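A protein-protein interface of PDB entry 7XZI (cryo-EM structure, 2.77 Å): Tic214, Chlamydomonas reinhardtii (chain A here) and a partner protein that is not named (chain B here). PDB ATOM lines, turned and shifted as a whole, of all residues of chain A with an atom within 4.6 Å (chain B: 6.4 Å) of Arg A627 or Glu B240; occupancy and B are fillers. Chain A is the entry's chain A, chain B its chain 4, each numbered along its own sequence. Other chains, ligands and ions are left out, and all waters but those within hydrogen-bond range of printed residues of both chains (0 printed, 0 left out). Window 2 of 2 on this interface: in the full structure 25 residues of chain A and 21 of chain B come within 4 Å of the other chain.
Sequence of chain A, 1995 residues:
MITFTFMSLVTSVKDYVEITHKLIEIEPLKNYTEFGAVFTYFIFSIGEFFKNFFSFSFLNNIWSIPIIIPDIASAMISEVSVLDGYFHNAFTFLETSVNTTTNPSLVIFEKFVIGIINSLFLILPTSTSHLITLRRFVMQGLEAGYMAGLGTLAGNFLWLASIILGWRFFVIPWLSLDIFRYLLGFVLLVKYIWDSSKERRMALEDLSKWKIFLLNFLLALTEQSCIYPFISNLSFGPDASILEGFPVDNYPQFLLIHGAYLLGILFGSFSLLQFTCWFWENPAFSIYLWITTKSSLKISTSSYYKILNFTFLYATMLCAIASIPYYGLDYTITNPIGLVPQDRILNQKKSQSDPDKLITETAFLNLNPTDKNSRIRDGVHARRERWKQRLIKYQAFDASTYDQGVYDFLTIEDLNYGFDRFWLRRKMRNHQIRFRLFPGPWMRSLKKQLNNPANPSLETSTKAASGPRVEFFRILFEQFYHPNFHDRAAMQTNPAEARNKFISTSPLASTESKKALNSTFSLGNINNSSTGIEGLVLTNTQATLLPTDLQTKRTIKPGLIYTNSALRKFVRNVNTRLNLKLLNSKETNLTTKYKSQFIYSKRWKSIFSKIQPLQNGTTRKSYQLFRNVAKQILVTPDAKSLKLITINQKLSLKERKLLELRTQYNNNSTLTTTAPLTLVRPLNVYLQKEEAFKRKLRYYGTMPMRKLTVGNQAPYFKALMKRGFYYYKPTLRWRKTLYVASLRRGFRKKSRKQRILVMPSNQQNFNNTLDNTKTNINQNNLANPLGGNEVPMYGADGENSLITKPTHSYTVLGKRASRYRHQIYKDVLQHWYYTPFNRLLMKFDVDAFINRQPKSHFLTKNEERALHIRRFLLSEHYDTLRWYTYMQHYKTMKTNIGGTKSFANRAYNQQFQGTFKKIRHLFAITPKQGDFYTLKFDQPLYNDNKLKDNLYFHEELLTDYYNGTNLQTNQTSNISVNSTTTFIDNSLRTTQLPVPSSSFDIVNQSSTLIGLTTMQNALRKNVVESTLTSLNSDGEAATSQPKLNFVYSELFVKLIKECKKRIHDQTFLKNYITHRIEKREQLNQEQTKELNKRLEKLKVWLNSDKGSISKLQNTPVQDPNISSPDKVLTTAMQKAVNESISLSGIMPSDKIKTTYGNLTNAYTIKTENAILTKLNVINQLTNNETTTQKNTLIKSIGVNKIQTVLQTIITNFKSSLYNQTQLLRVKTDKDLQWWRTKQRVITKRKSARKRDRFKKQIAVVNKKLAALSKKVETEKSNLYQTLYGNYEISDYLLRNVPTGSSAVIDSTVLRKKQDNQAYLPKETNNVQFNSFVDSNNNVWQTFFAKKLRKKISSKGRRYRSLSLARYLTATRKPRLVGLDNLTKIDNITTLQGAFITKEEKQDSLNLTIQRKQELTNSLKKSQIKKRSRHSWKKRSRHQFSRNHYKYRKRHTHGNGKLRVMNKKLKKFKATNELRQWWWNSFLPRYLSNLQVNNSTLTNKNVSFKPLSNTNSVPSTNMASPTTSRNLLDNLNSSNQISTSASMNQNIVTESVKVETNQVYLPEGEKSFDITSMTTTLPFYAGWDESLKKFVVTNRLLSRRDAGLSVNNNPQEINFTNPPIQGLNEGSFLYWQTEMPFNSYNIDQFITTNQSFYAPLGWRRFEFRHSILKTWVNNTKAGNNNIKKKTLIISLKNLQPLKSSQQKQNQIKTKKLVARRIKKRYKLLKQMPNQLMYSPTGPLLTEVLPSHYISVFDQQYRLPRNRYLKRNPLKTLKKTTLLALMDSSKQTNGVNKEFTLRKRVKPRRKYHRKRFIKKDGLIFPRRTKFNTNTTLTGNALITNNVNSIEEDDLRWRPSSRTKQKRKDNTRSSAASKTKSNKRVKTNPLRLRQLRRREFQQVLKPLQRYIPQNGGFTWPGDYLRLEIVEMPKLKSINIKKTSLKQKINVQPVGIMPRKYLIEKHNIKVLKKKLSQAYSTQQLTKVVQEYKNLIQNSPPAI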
ATOM      1  N   TYR A 623      15.073  -8.177 -19.513  1.00  0.00           N
ATOM      2  CA  TYR A 623      13.778  -8.558 -20.062  1.00  0.00           C
ATOM      3  C   TYR A 623      12.849  -7.358 -20.162  1.00  0.00           C
ATOM      4  O   TYR A 623      12.099  -7.230 -21.133  1.00  0.00           O
ATOM      5  CB  TYR A 623      13.151  -9.658 -19.207  1.00  0.00           C
ATOM      6  CG  TYR A 623      11.672  -9.858 -19.454  1.00  0.00           C
ATOM      7  CD1 TYR A 623      11.219 -10.491 -20.603  1.00  0.00           C
ATOM      8  CD2 TYR A 623      10.729  -9.418 -18.533  1.00  0.00           C
ATOM      9  CE1 TYR A 623       9.869 -10.675 -20.831  1.00  0.00           C
ATOM     10  CE2 TYR A 623       9.378  -9.599 -18.753  1.00  0.00           C
ATOM     11  CZ  TYR A 623       8.954 -10.229 -19.904  1.00  0.00           C
ATOM     12  OH  TYR A 623       7.609 -10.412 -20.129  1.00  0.00           O
ATOM     13  N   GLN A 624      12.878  -6.469 -19.166  1.00  0.00           N
ATOM     14  CA  GLN A 624      12.047  -5.271 -19.222  1.00  0.00           C
ATOM     15  C   GLN A 624      12.450  -4.374 -20.384  1.00  0.00           C
ATOM     16  O   GLN A 624      11.589  -3.860 -21.109  1.00  0.00           O
ATOM     17  CB  GLN A 624      12.137  -4.504 -17.903  1.00  0.00           C
ATOM     18  CG  GLN A 624      11.351  -3.200 -17.896  1.00  0.00           C
ATOM     19  CD  GLN A 624      11.686  -2.317 -16.709  1.00  0.00           C
ATOM     20  OE1 GLN A 624      12.571  -2.635 -15.915  1.00  0.00           O
ATOM     21  NE2 GLN A 624      10.979  -1.200 -16.585  1.00  0.00           N
ATOM     22  N   LEU A 625      13.756  -4.177 -20.579  1.00  0.00           N
ATOM     23  CA  LEU A 625      14.212  -3.357 -21.699  1.00  0.00           C
ATOM     24  C   LEU A 625      13.786  -3.961 -23.033  1.00  0.00           C
ATOM     25  O   LEU A 625      13.246  -3.258 -23.903  1.00  0.00           O
ATOM     26  CB  LEU A 625      15.732  -3.196 -21.651  1.00  0.00           C
ATOM     27  CG  LEU A 625      16.316  -2.442 -20.457  1.00  0.00           C
ATOM     28  CD1 LEU A 625      17.836  -2.463 -20.505  1.00  0.00           C
ATOM     29  CD2 LEU A 625      15.797  -1.015 -20.427  1.00  0.00           C
ATOM     30  N   PHE A 626      14.013  -5.265 -23.208  1.00  0.00           N
ATOM     31  CA  PHE A 626      13.641  -5.906 -24.463  1.00  0.00           C
ATOM     32  C   PHE A 626      12.135  -5.868 -24.677  1.00  0.00           C
ATOM     33  O   PHE A 626      11.671  -5.674 -25.803  1.00  0.00           O
ATOM     34  CB  PHE A 626      14.144  -7.347 -24.507  1.00  0.00           C
ATOM     35  CG  PHE A 626      13.747  -8.080 -25.756  1.00  0.00           C
ATOM     36  CD1 PHE A 626      14.431  -7.873 -26.941  1.00  0.00           C
ATOM     37  CD2 PHE A 626      12.680  -8.963 -25.750  1.00  0.00           C
ATOM     38  CE1 PHE A 626      14.065  -8.537 -28.093  1.00  0.00           C
ATOM     39  CE2 PHE A 626      12.310  -9.632 -26.900  1.00  0.00           C
ATOM     40  CZ  PHE A 626      13.004  -9.418 -28.073  1.00  0.00           C
ATOM     41  N   ARG A 627      11.356  -6.068 -23.611  1.00  0.00           N
ATOM     42  CA  ARG A 627       9.905  -6.020 -23.726  1.00  0.00           C
ATOM     43  C   ARG A 627       9.433  -4.631 -24.128  1.00  0.00           C
ATOM     44  O   ARG A 627       8.553  -4.494 -24.984  1.00  0.00           O
ATOM     45  CB  ARG A 627       9.267  -6.452 -22.407  1.00  0.00           C
ATOM     46  CG  ARG A 627       7.765  -6.247 -22.338  1.00  0.00           C
ATOM     47  CD  ARG A 627       7.170  -6.968 -21.140  1.00  0.00           C
ATOM     48  NE  ARG A 627       7.887  -6.667 -19.910  1.00  0.00           N
ATOM     49  CZ  ARG A 627       7.563  -5.688 -19.071  1.00  0.00           C
ATOM     50  NH1 ARG A 627       6.527  -4.898 -19.297  1.00  0.00           N
ATOM     51  NH2 ARG A 627       8.298  -5.501 -17.979  1.00  0.00           N
ATOM     52  N   ASN A 628      10.010  -3.587 -23.529  1.00  0.00           N
ATOM     53  CA  ASN A 628       9.657  -2.226 -23.920  1.00  0.00           C
ATOM     54  C   ASN A 628       9.938  -1.996 -25.398  1.00  0.00           C
ATOM     55  O   ASN A 628       9.066  -1.531 -26.145  1.00  0.00           O
ATOM     56  CB  ASN A 628      10.424  -1.215 -23.064  1.00  0.00           C
ATOM     57  CG  ASN A 628      10.006  -1.242 -21.608  1.00  0.00           C
ATOM     58  OD1 ASN A 628       9.291  -2.144 -21.172  1.00  0.00           O
ATOM     59  ND2 ASN A 628      10.452  -0.250 -20.845  1.00  0.00           N
ATOM     60  N   VAL A 629      11.147  -2.348 -25.846  1.00  0.00           N
ATOM     61  CA  VAL A 629      11.512  -2.091 -27.238  1.00  0.00           C
ATOM     62  C   VAL A 629      10.629  -2.895 -28.188  1.00  0.00           C
ATOM     63  O   VAL A 629      10.150  -2.375 -29.205  1.00  0.00           O
ATOM     64  CB  VAL A 629      13.008  -2.381 -27.464  1.00  0.00           C
ATOM     65  CG1 VAL A 629      13.382  -2.118 -28.912  1.00  0.00           C
ATOM     66  CG2 VAL A 629      13.851  -1.523 -26.540  1.00  0.00           C
ATOM     67  N   ALA A 630      10.392  -4.171 -27.872  1.00  0.00           N
ATOM     68  CA  ALA A 630       9.595  -5.025 -28.747  1.00  0.00           C
ATOM     69  C   ALA A 630       8.146  -4.563 -28.814  1.00  0.00           C
ATOM     70  O   ALA A 630       7.556  -4.519 -29.900  1.00  0.00           O
ATOM     71  CB  ALA A 630       9.675  -6.476 -28.277  1.00  0.00           C
ATOM     72  N   LYS A 631       7.548  -4.219 -27.669  1.00  0.00           N
ATOM     73  CA  LYS A 631       6.184  -3.704 -27.685  1.00  0.00           C
ATOM     74  C   LYS A 631       6.101  -2.387 -28.437  1.00  0.00           C
ATOM     75  O   LYS A 631       5.075  -2.090 -29.059  1.00  0.00           O
ATOM     76  CB  LYS A 631       5.661  -3.528 -26.259  1.00  0.00           C
ATOM     77  CG  LYS A 631       5.421  -4.826 -25.506  1.00  0.00           C
ATOM     78  CD  LYS A 631       4.711  -4.569 -24.186  1.00  0.00           C
ATOM     79  CE  LYS A 631       5.453  -3.540 -23.348  1.00  0.00           C
ATOM     80  NZ  LYS A 631       4.719  -3.206 -22.096  1.00  0.00           N
ATOM     81  N   LYS A 640      -2.369 -10.570 -29.579  1.00  0.00           N
ATOM     82  CA  LYS A 640      -2.924 -10.669 -28.233  1.00  0.00           C
ATOM     83  C   LYS A 640      -1.884 -10.309 -27.178  1.00  0.00           C
ATOM     84  O   LYS A 640      -2.165  -9.541 -26.252  1.00  0.00           O
ATOM     85  CB  LYS A 640      -3.469 -12.077 -27.994  1.00  0.00           C
ATOM     86  N   SER A 641      -0.677 -10.856 -27.302  1.00  0.00           N
ATOM     87  CA  SER A 641       0.368 -10.617 -26.317  1.00  0.00           C
ATOM     88  C   SER A 641       1.726 -10.853 -26.959  1.00  0.00           C
ATOM     89  O   SER A 641       1.847 -11.572 -27.955  1.00  0.00           O
ATOM     90  CB  SER A 641       0.191 -11.512 -25.087  1.00  0.00           C
ATOM     91  OG  SER A 641       1.289 -11.384 -24.201  1.00  0.00           O
ATOM     92  N   LEU A 642       2.751 -10.235 -26.366  1.00  0.00           N
ATOM     93  CA  LEU A 642       4.118 -10.442 -26.832  1.00  0.00           C
ATOM     94  C   LEU A 642       4.576 -11.875 -26.583  1.00  0.00           C
ATOM     95  O   LEU A 642       5.193 -12.497 -27.455  1.00  0.00           O
ATOM     96  CB  LEU A 642       5.061  -9.451 -26.149  1.00  0.00           C
ATOM     97  CG  LEU A 642       6.564  -9.675 -26.328  1.00  0.00           C
ATOM     98  CD1 LEU A 642       6.959  -9.566 -27.791  1.00  0.00           C
ATOM     99  CD2 LEU A 642       7.358  -8.692 -25.481  1.00  0.00           C
ATOM    100  N   LYS A 643       4.288 -12.413 -25.395  1.00  0.00           N
ATOM    101  CA  LYS A 643       4.686 -13.783 -25.092  1.00  0.00           C
ATOM    102  C   LYS A 643       3.950 -14.780 -25.977  1.00  0.00           C
ATOM    103  O   LYS A 643       4.533 -15.775 -26.424  1.00  0.00           O
ATOM    104  CB  LYS A 643       4.440 -14.083 -23.612  1.00  0.00           C
ATOM    105  CG  LYS A 643       5.080 -15.375 -23.131  1.00  0.00           C
ATOM    106  CD  LYS A 643       4.921 -15.548 -21.629  1.00  0.00           C
ATOM    107  CE  LYS A 643       5.556 -14.396 -20.867  1.00  0.00           C
ATOM    108  NZ  LYS A 643       5.375 -14.539 -19.396  1.00  0.00           N
ATOM    109  N   VAL B 234      -3.294 -15.592 -16.467  1.00  0.00           N
ATOM    110  CA  VAL B 234      -2.474 -14.593 -15.782  1.00  0.00           C
ATOM    111  C   VAL B 234      -1.065 -14.560 -16.367  1.00  0.00           C
ATOM    112  O   VAL B 234      -0.500 -13.489 -16.613  1.00  0.00           O
ATOM    113  CB  VAL B 234      -2.452 -14.866 -14.267  1.00  0.00           C
ATOM    114  CG1 VAL B 234      -1.417 -13.987 -13.583  1.00  0.00           C
ATOM    115  CG2 VAL B 234      -3.828 -14.630 -13.666  1.00  0.00           C
ATOM    116  N   ASP B 235      -0.478 -15.737 -16.597  1.00  0.00           N
ATOM    117  CA  ASP B 235       0.923 -15.817 -17.001  1.00  0.00           C
ATOM    118  C   ASP B 235       1.151 -15.225 -18.387  1.00  0.00           C
ATOM    119  O   ASP B 235       2.106 -14.468 -18.601  1.00  0.00           O
ATOM    120  CB  ASP B 235       1.393 -17.271 -16.953  1.00  0.00           C
ATOM    121  CG  ASP B 235       2.737 -17.476 -17.624  1.00  0.00           C
ATOM    122  OD1 ASP B 235       3.756 -16.993 -17.087  1.00  0.00           O
ATOM    123  OD2 ASP B 235       2.775 -18.126 -18.690  1.00  0.00           O
ATOM    124  N   TYR B 236       0.288 -15.560 -19.348  1.00  0.00           N
ATOM    125  CA  TYR B 236       0.566 -15.201 -20.736  1.00  0.00           C
ATOM    126  C   TYR B 236       0.113 -13.783 -21.065  1.00  0.00           C
ATOM    127  O   TYR B 236       0.771 -13.086 -21.846  1.00  0.00           O
ATOM    128  CB  TYR B 236      -0.095 -16.206 -21.681  1.00  0.00           C
ATOM    129  CG  TYR B 236       0.695 -17.482 -21.871  1.00  0.00           C
ATOM    130  CD1 TYR B 236       1.743 -17.542 -22.780  1.00  0.00           C
ATOM    131  CD2 TYR B 236       0.392 -18.625 -21.146  1.00  0.00           C
ATOM    132  CE1 TYR B 236       2.469 -18.705 -22.958  1.00  0.00           C
ATOM    133  CE2 TYR B 236       1.112 -19.792 -21.318  1.00  0.00           C
ATOM    134  CZ  TYR B 236       2.149 -19.827 -22.225  1.00  0.00           C
ATOM    135  OH  TYR B 236       2.867 -20.987 -22.398  1.00  0.00           O
ATOM    136  N   ARG B 237      -1.002 -13.332 -20.486  1.00  0.00           N
ATOM    137  CA  ARG B 237      -1.632 -12.094 -20.923  1.00  0.00           C
ATOM    138  C   ARG B 237      -1.558 -10.948 -19.925  1.00  0.00           C
ATOM    139  O   ARG B 237      -1.839  -9.808 -20.307  1.00  0.00           O
ATOM    140  CB  ARG B 237      -3.107 -12.343 -21.268  1.00  0.00           C
ATOM    141  CG  ARG B 237      -3.315 -13.333 -22.400  1.00  0.00           C
ATOM    142  CD  ARG B 237      -4.792 -13.607 -22.632  1.00  0.00           C
ATOM    143  NE  ARG B 237      -5.526 -12.395 -22.959  1.00  0.00           N
ATOM    144  CZ  ARG B 237      -5.750 -11.963 -24.196  1.00  0.00           C
ATOM    145  NH1 ARG B 237      -5.317 -12.633 -25.251  1.00  0.00           N
ATOM    146  NH2 ARG B 237      -6.426 -10.833 -24.375  1.00  0.00           N
ATOM    147  N   ILE B 238      -1.196 -11.206 -18.671  1.00  0.00           N
ATOM    148  CA  ILE B 238      -1.206 -10.167 -17.650  1.00  0.00           C
ATOM    149  C   ILE B 238       0.187  -9.834 -17.122  1.00  0.00           C
ATOM    150  O   ILE B 238       0.428  -8.672 -16.759  1.00  0.00           O
ATOM    151  CB  ILE B 238      -2.147 -10.549 -16.486  1.00  0.00           C
ATOM    152  CG1 ILE B 238      -3.568 -10.768 -17.009  1.00  0.00           C
ATOM    153  CG2 ILE B 238      -2.146  -9.485 -15.395  1.00  0.00           C
ATOM    154  CD1 ILE B 238      -4.614 -10.881 -15.923  1.00  0.00           C
ATOM    155  N   GLU B 239       1.117 -10.791 -17.109  1.00  0.00           N
ATOM    156  CA  GLU B 239       2.430 -10.549 -16.517  1.00  0.00           C
ATOM    157  C   GLU B 239       3.183  -9.440 -17.245  1.00  0.00           C
ATOM    158  O   GLU B 239       3.860  -8.623 -16.612  1.00  0.00           O
ATOM    159  CB  GLU B 239       3.245 -11.841 -16.521  1.00  0.00           C
ATOM    160  CG  GLU B 239       4.676 -11.680 -16.040  1.00  0.00           C
ATOM    161  CD  GLU B 239       5.468 -12.966 -16.153  1.00  0.00           C
ATOM    162  OE1 GLU B 239       4.875 -14.048 -15.962  1.00  0.00           O
ATOM    163  OE2 GLU B 239       6.679 -12.895 -16.445  1.00  0.00           O
ATOM    164  N   GLU B 240       3.081  -9.400 -18.577  1.00  0.00           N
ATOM    165  CA  GLU B 240       3.818  -8.403 -19.347  1.00  0.00           C
ATOM    166  C   GLU B 240       3.358  -6.986 -19.031  1.00  0.00           C
ATOM    167  O   GLU B 240       4.180  -6.063 -18.987  1.00  0.00           O
ATOM    168  CB  GLU B 240       3.678  -8.687 -20.843  1.00  0.00           C
ATOM    169  CG  GLU B 240       2.242  -8.774 -21.331  1.00  0.00           C
ATOM    170  CD  GLU B 240       2.141  -8.834 -22.841  1.00  0.00           C
ATOM    171  OE1 GLU B 240       3.191  -8.952 -23.504  1.00  0.00           O
ATOM    172  OE2 GLU B 240       1.009  -8.763 -23.365  1.00  0.00           O
ATOM    173  N   ASN B 241       2.057  -6.787 -18.813  1.00  0.00           N
ATOM    174  CA  ASN B 241       1.530  -5.455 -18.548  1.00  0.00           C
ATOM    175  C   ASN B 241       1.727  -5.019 -17.101  1.00  0.00           C
ATOM    176  O   ASN B 241       1.470  -3.853 -16.782  1.00  0.00           O
ATOM    177  CB  ASN B 241       0.043  -5.398 -18.907  1.00  0.00           C
ATOM    178  CG  ASN B 241      -0.222  -5.773 -20.354  1.00  0.00           C
ATOM    179  OD1 ASN B 241       0.656  -5.652 -21.208  1.00  0.00           O
ATOM    180  ND2 ASN B 241      -1.437  -6.228 -20.634  1.00  0.00           N
ATOM    181  N   ILE B 242       2.167  -5.919 -16.229  1.00  0.00           N
ATOM    182  CA  ILE B 242       2.398  -5.555 -14.826  1.00  0.00           C
ATOM    183  C   ILE B 242       3.544  -4.552 -14.748  1.00  0.00           C
ATOM    184  O   ILE B 242       4.593  -4.759 -15.390  1.00  0.00           O
ATOM    185  CB  ILE B 242       2.702  -6.810 -13.988  1.00  0.00           C
ATOM    186  CG1 ILE B 242       1.462  -7.699 -13.887  1.00  0.00           C
ATOM    187  CG2 ILE B 242       3.189  -6.428 -12.602  1.00  0.00           C
ATOM    188  CD1 ILE B 242       0.279  -7.021 -13.232  1.00  0.00           C
ATOM    189  N   PRO B 243       3.403  -3.456 -14.001  1.00  0.00           N
ATOM    190  CA  PRO B 243       4.494  -2.477 -13.915  1.00  0.00           C
ATOM    191  C   PRO B 243       5.724  -3.056 -13.230  1.00  0.00           C
ATOM    192  O   PRO B 243       5.635  -3.961 -12.399  1.00  0.00           O
ATOM    193  CB  PRO B 243       3.881  -1.335 -13.096  1.00  0.00           C
ATOM    194  CG  PRO B 243       2.754  -1.963 -12.344  1.00  0.00           C
ATOM    195  CD  PRO B 243       2.213  -3.028 -13.248  1.00  0.00           C
ATOM    196  N   SER B 244       6.888  -2.513 -13.597  1.00  0.00           N
ATOM    197  CA  SER B 244       8.153  -3.076 -13.132  1.00  0.00           C
ATOM    198  C   SER B 244       8.399  -2.787 -11.655  1.00  0.00           C
ATOM    199  O   SER B 244       8.978  -3.617 -10.945  1.00  0.00           O
ATOM    200  CB  SER B 244       9.306  -2.538 -13.980  1.00  0.00           C
ATOM    201  OG  SER B 244      10.553  -3.033 -13.523  1.00  0.00           O
ATOM    202  N   TRP B 247       7.711  -5.308  -8.986  1.00  0.00           N
ATOM    203  CA  TRP B 247       8.484  -6.547  -8.956  1.00  0.00           C
ATOM    204  C   TRP B 247       9.631  -6.468  -7.954  1.00  0.00           C
ATOM    205  O   TRP B 247      10.004  -7.479  -7.348  1.00  0.00           O
ATOM    206  CB  TRP B 247       9.009  -6.879 -10.353  1.00  0.00           C
ATOM    207  CG  TRP B 247       7.924  -7.236 -11.325  1.00  0.00           C
ATOM    208  CD1 TRP B 247       7.473  -6.479 -12.367  1.00  0.00           C
ATOM    209  CD2 TRP B 247       7.142  -8.438 -11.334  1.00  0.00           C
ATOM    210  NE1 TRP B 247       6.464  -7.137 -13.028  1.00  0.00           N
ATOM    211  CE2 TRP B 247       6.241  -8.342 -12.414  1.00  0.00           C
ATOM    212  CE3 TRP B 247       7.118  -9.585 -10.536  1.00  0.00           C
ATOM    213  CZ2 TRP B 247       5.327  -9.348 -12.715  1.00  0.00           C
ATOM    214  CZ3 TRP B 247       6.209 -10.584 -10.838  1.00  0.00           C
ATOM    215  CH2 TRP B 247       5.326 -10.458 -11.918  1.00  0.00           C
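NZ of Lys A643 lies within salt-bridge range of OD1 of Asp B235 (3.7 Å). The side-chain amino group of Lys A643 is in salt-bridge range of the side-chain carboxylate of Glu B239, 3.5 Å away. N of Leu A642 is in hydrogen-bond range of OE1 of Glu B240. The backbone carbonyl oxygen (O) of Tyr B236 is in hydrogen-bond range of the side-chain hydroxyl (OG) of Ser A641 (3.0 Å). The side-chain carboxylate (OE2) of Glu B240 is in hydrogen-bond range of the side-chain hydroxyl (OG) of Ser A641, 2.8 Å away. The side-chain hydroxyl (OG) of Ser B244 lies within hydrogen-bond range of the side-chain amide oxygen (OE1) of Gln A624, at 3.2 Å. NH1 of Arg A627 is in hydrogen-bond range of O of Glu B240, 2.6 Å away.
N of Lys A643 sits close to OG of Ser A641, 3.4 Å away. The backbone carbonyl oxygen (O) of Gln A624 sits close to the side-chain amide oxygen (OD1) of Asn A628. O of Val B234 is in hydrogen-bond range of N of Glu B239, 3.2 Å away.
Among the printed residues, merely in contact across the chains: Lys A640 with Arg B237 (3.4 Å) and Lys A643 with Tyr B236 (3.9 Å).
Arg A627 touches just one residue of chain B: Glu B240. Of chain A, only Arg A627 (2.6 Å), Ser A641 (2.8 Å) and Leu A642 (3.2 Å) come within 4 Å of Glu B240. Printed residues of chain B within 4 Å of Lys A643: Asp B235, Tyr B236 and Glu B239. Of the printed residues of chain B, Gln A624 touches Ser B244. Ala A630 touches none of the printed residues of chain B. The nearest residue of chain B that does not touch Arg A627 is Ile B242 (4.4 Å). The nearest residue of chain A that does not touch Glu B240 is Lys A643 (4.1 Å). The nearest printed residue of chain A that does not touch Asp B235 is Ser A641 (6.4 Å).
Along chain B the printed residues that touch a printed residue of chain A span positions 235 to 244. Of the 13 printed residues of chain A, 6 touch a printed residue of chain B. Among the printed residues, 9 pairs touch across the chains. Among the printed residues, Asp or Glu carboxylates within 4 Å of a Lys or Arg side-chain nitrogen of the other chain: Lys A643 with Asp B235 (3.7 Å) and Lys A643 with Glu B239 (3.5 Å).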
